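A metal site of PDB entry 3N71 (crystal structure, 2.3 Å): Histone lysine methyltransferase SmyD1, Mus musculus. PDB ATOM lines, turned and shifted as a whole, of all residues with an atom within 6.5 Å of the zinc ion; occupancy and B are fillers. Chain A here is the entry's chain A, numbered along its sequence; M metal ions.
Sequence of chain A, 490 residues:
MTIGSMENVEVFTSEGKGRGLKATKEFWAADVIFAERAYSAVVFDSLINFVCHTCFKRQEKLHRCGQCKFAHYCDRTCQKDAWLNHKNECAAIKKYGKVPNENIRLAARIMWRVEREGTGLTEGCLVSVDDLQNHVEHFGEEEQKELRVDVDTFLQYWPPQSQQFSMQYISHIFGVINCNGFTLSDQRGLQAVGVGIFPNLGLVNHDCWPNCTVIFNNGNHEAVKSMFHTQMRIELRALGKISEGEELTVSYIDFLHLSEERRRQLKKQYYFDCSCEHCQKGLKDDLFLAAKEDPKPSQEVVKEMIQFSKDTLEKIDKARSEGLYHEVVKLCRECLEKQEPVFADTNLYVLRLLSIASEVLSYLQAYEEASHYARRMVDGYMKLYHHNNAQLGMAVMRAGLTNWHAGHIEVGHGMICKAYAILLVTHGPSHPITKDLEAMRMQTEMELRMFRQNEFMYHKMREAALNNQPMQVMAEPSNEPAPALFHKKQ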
ATOM      1  N   CYS A  52      31.191 -25.680 -14.897  1.00  0.00           N
ATOM      2  CA  CYS A  52      29.955 -25.336 -15.576  1.00  0.00           C
ATOM      3  C   CYS A  52      28.733 -25.525 -14.628  1.00  0.00           C
ATOM      4  O   CYS A  52      28.558 -26.591 -14.021  1.00  0.00           O
ATOM      5  CB  CYS A  52      29.766 -26.201 -16.821  1.00  0.00           C
ATOM      6  SG  CYS A  52      28.206 -25.856 -17.686  1.00  0.00           S
ATOM      7  N   HIS A  53      27.894 -24.504 -14.516  1.00  0.00           N
ATOM      8  CA  HIS A  53      26.726 -24.541 -13.641  1.00  0.00           C
ATOM      9  C   HIS A  53      25.600 -25.375 -14.190  1.00  0.00           C
ATOM     10  O   HIS A  53      24.613 -25.648 -13.514  1.00  0.00           O
ATOM     11  CB  HIS A  53      26.219 -23.122 -13.388  1.00  0.00           C
ATOM     12  CG  HIS A  53      27.043 -22.373 -12.375  1.00  0.00           C
ATOM     13  ND1 HIS A  53      28.416 -22.416 -12.373  1.00  0.00           N
ATOM     14  CD2 HIS A  53      26.682 -21.579 -11.342  1.00  0.00           C
ATOM     15  CE1 HIS A  53      28.869 -21.674 -11.378  1.00  0.00           C
ATOM     16  NE2 HIS A  53      27.833 -21.163 -10.737  1.00  0.00           N
ATOM     17  N   THR A  54      25.748 -25.791 -15.436  1.00  0.00           N
ATOM     18  CA  THR A  54      24.739 -26.605 -16.083  1.00  0.00           C
ATOM     19  C   THR A  54      25.145 -28.050 -16.078  1.00  0.00           C
ATOM     20  O   THR A  54      24.359 -28.938 -15.748  1.00  0.00           O
ATOM     21  CB  THR A  54      24.533 -26.180 -17.542  1.00  0.00           C
ATOM     22  OG1 THR A  54      23.908 -24.894 -17.567  1.00  0.00           O
ATOM     23  CG2 THR A  54      23.689 -27.213 -18.308  1.00  0.00           C
ATOM     24  N   CYS A  55      26.404 -28.293 -16.449  1.00  0.00           N
ATOM     25  CA  CYS A  55      26.852 -29.664 -16.547  1.00  0.00           C
ATOM     26  C   CYS A  55      27.939 -30.169 -15.593  1.00  0.00           C
ATOM     27  O   CYS A  55      28.266 -31.352 -15.616  1.00  0.00           O
ATOM     28  CB  CYS A  55      27.212 -30.002 -18.008  1.00  0.00           C
ATOM     29  SG  CYS A  55      28.990 -29.852 -18.411  1.00  0.00           S
ATOM     30  N   PHE A  56      28.494 -29.288 -14.769  1.00  0.00           N
ATOM     31  CA  PHE A  56      29.503 -29.660 -13.785  1.00  0.00           C
ATOM     32  C   PHE A  56      30.851 -30.161 -14.297  1.00  0.00           C
ATOM     33  O   PHE A  56      31.589 -30.837 -13.572  1.00  0.00           O
ATOM     34  CB  PHE A  56      28.872 -30.658 -12.809  1.00  0.00           C
ATOM     35  CG  PHE A  56      27.713 -30.097 -12.071  1.00  0.00           C
ATOM     36  CD1 PHE A  56      27.923 -29.217 -11.009  1.00  0.00           C
ATOM     37  CD2 PHE A  56      26.413 -30.294 -12.532  1.00  0.00           C
ATOM     38  CE1 PHE A  56      26.848 -28.569 -10.405  1.00  0.00           C
ATOM     39  CE2 PHE A  56      25.336 -29.653 -11.934  1.00  0.00           C
ATOM     40  CZ  PHE A  56      25.556 -28.770 -10.863  1.00  0.00           C
ATOM     41  N   LYS A  57      31.174 -29.818 -15.532  1.00  0.00           N
ATOM     42  CA  LYS A  57      32.466 -30.182 -16.106  1.00  0.00           C
ATOM     43  C   LYS A  57      33.463 -29.089 -15.801  1.00  0.00           C
ATOM     44  O   LYS A  57      33.099 -27.927 -15.707  1.00  0.00           O
ATOM     45  CB  LYS A  57      32.363 -30.357 -17.625  1.00  0.00           C
ATOM     46  CG  LYS A  57      31.504 -31.511 -18.051  1.00  0.00           C
ATOM     47  CD  LYS A  57      31.461 -31.665 -19.570  1.00  0.00           C
ATOM     48  CE  LYS A  57      30.581 -32.831 -19.990  1.00  0.00           C
ATOM     49  NZ  LYS A  57      30.570 -33.042 -21.453  1.00  0.00           N
ATOM     50  N   GLN A  59      36.845 -27.010 -16.911  1.00  0.00           N
ATOM     51  CA  GLN A  59      37.325 -26.562 -18.217  1.00  0.00           C
ATOM     52  C   GLN A  59      38.127 -25.290 -18.100  1.00  0.00           C
ATOM     53  O   GLN A  59      37.870 -24.472 -17.227  1.00  0.00           O
ATOM     54  CB  GLN A  59      36.168 -26.372 -19.186  1.00  0.00           C
ATOM     55  CG  GLN A  59      35.914 -27.576 -20.072  1.00  0.00           C
ATOM     56  CD  GLN A  59      34.451 -27.735 -20.375  1.00  0.00           C
ATOM     57  OE1 GLN A  59      33.657 -26.843 -20.080  1.00  0.00           O
ATOM     58  NE2 GLN A  59      34.078 -28.860 -20.978  1.00  0.00           N
ATOM     59  N   HIS A  72      28.532 -19.768 -14.731  1.00  0.00           N
ATOM     60  CA  HIS A  72      29.537 -19.960 -15.771  1.00  0.00           C
ATOM     61  C   HIS A  72      29.133 -21.190 -16.572  1.00  0.00           C
ATOM     62  O   HIS A  72      28.528 -22.122 -16.032  1.00  0.00           O
ATOM     63  CB  HIS A  72      30.923 -20.153 -15.166  1.00  0.00           C
ATOM     64  CG  HIS A  72      31.449 -18.940 -14.468  1.00  0.00           C
ATOM     65  ND1 HIS A  72      32.792 -18.629 -14.443  1.00  0.00           N
ATOM     66  CD2 HIS A  72      30.825 -17.977 -13.761  1.00  0.00           C
ATOM     67  CE1 HIS A  72      32.969 -17.534 -13.735  1.00  0.00           C
ATOM     68  NE2 HIS A  72      31.794 -17.112 -13.303  1.00  0.00           N
ATOM     69  N   TYR A  73      29.472 -21.193 -17.850  1.00  0.00           N
ATOM     70  CA  TYR A  73      29.090 -22.307 -18.700  1.00  0.00           C
ATOM     71  C   TYR A  73      30.165 -22.705 -19.696  1.00  0.00           C
ATOM     72  O   TYR A  73      31.118 -21.962 -19.946  1.00  0.00           O
ATOM     73  CB  TYR A  73      27.816 -21.945 -19.450  1.00  0.00           C
ATOM     74  CG  TYR A  73      26.692 -21.443 -18.559  1.00  0.00           C
ATOM     75  CD1 TYR A  73      25.958 -22.325 -17.762  1.00  0.00           C
ATOM     76  CD2 TYR A  73      26.371 -20.087 -18.505  1.00  0.00           C
ATOM     77  CE1 TYR A  73      24.914 -21.853 -16.944  1.00  0.00           C
ATOM     78  CE2 TYR A  73      25.343 -19.617 -17.706  1.00  0.00           C
ATOM     79  CZ  TYR A  73      24.617 -20.498 -16.929  1.00  0.00           C
ATOM     80  OH  TYR A  73      23.607 -20.014 -16.122  1.00  0.00           O
ATOM     81  N   CYS A  74      30.013 -23.903 -20.259  1.00  0.00           N
ATOM     82  CA  CYS A  74      30.947 -24.414 -21.247  1.00  0.00           C
ATOM     83  C   CYS A  74      30.635 -23.671 -22.552  1.00  0.00           C
ATOM     84  O   CYS A  74      31.529 -23.133 -23.207  1.00  0.00           O
ATOM     85  CB  CYS A  74      30.730 -25.903 -21.475  1.00  0.00           C
ATOM     86  SG  CYS A  74      30.816 -26.969 -20.024  1.00  0.00           S
ATOM     87  N   ASP A  75      29.350 -23.661 -22.913  1.00  0.00           N
ATOM     88  CA  ASP A  75      28.877 -23.022 -24.135  1.00  0.00           C
ATOM     89  C   ASP A  75      27.655 -22.171 -23.891  1.00  0.00           C
ATOM     90  O   ASP A  75      27.162 -22.044 -22.767  1.00  0.00           O
ATOM     91  CB  ASP A  75      28.424 -24.042 -25.182  1.00  0.00           C
ATOM     92  CG  ASP A  75      29.417 -25.149 -25.405  1.00  0.00           C
ATOM     93  OD1 ASP A  75      30.629 -24.857 -25.455  1.00  0.00           O
ATOM     94  OD2 ASP A  75      28.978 -26.314 -25.556  1.00  0.00           O
ATOM     95  N   CYS A  78      25.123 -24.859 -22.968  1.00  0.00           N
ATOM     96  CA  CYS A  78      24.901 -25.184 -21.568  1.00  0.00           C
ATOM     97  C   CYS A  78      24.200 -24.003 -20.900  1.00  0.00           C
ATOM     98  O   CYS A  78      23.464 -24.173 -19.928  1.00  0.00           O
ATOM     99  CB  CYS A  78      26.224 -25.504 -20.854  1.00  0.00           C
ATOM    100  SG  CYS A  78      26.906 -27.143 -21.260  1.00  0.00           S
ATOM    101  N   HIS A 221      27.137 -33.113 -25.317  1.00  0.00           N
ATOM    102  CA  HIS A 221      26.324 -32.611 -26.412  1.00  0.00           C
ATOM    103  C   HIS A 221      27.200 -32.256 -27.622  1.00  0.00           C
ATOM    104  O   HIS A 221      28.019 -31.341 -27.568  1.00  0.00           O
ATOM    105  CB  HIS A 221      25.459 -31.417 -25.988  1.00  0.00           C
ATOM    106  CG  HIS A 221      26.235 -30.204 -25.569  1.00  0.00           C
ATOM    107  ND1 HIS A 221      26.454 -29.883 -24.248  1.00  0.00           N
ATOM    108  CD2 HIS A 221      26.853 -29.253 -26.295  1.00  0.00           C
ATOM    109  CE1 HIS A 221      27.168 -28.769 -24.184  1.00  0.00           C
ATOM    110  NE2 HIS A 221      27.426 -28.370 -25.415  1.00  0.00           N
ATOM    111  N   MET A 232      22.567 -35.717 -18.918  1.00  0.00           N
ATOM    112  CA  MET A 232      23.138 -35.626 -17.578  1.00  0.00           C
ATOM    113  C   MET A 232      22.184 -36.400 -16.687  1.00  0.00           C
ATOM    114  O   MET A 232      20.950 -36.243 -16.795  1.00  0.00           O
ATOM    115  CB  MET A 232      23.205 -34.175 -17.108  1.00  0.00           C
ATOM    116  CG  MET A 232      23.771 -34.044 -15.718  1.00  0.00           C
ATOM    117  SD  MET A 232      23.832 -32.343 -15.191  1.00  0.00           S
ATOM    118  CE  MET A 232      25.193 -31.870 -16.095  1.00  0.00           C
HETATM  119 ZN    ZN M   1      28.327 -27.621 -19.379  1.00  0.00          ZN
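The zinc ion is bound by the side-chain sulfur of Cys 78 (2.4 Å), the side-chain sulfur of Cys 52 (2.4 Å), the side-chain sulfur of Cys 55 (2.5 Å) and the side-chain sulfur of Cys 74 (2.7 Å).
The zinc ion has four donor atoms within binding distance.
The side-chain sulfur of Cys 55 sits close to the backbone NH of Lys 57, 3.6 Å away.
The side-chain sulfur (SG) of Cys 52 lies close to the backbone NH (N) of Thr 54, 3.3 Å away.
The backbone carbonyl oxygen (O) of Cys 78 sits at hydrogen-bond distance from the side-chain hydroxyl (OG1) of Thr 54 (2.5 Å).
The side-chain sulfur of Cys 74 lies close to the side-chain amide oxygen of Gln 59, at 2.8 Å.
N of Cys 52 sits at hydrogen-bond distance from O of Lys 57.
Of the 14 residues printed, 4 come within 4 Å of the zinc ion.
The nearest printed residue that does not touch the zinc ion is Thr 54 (4.5 Å).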
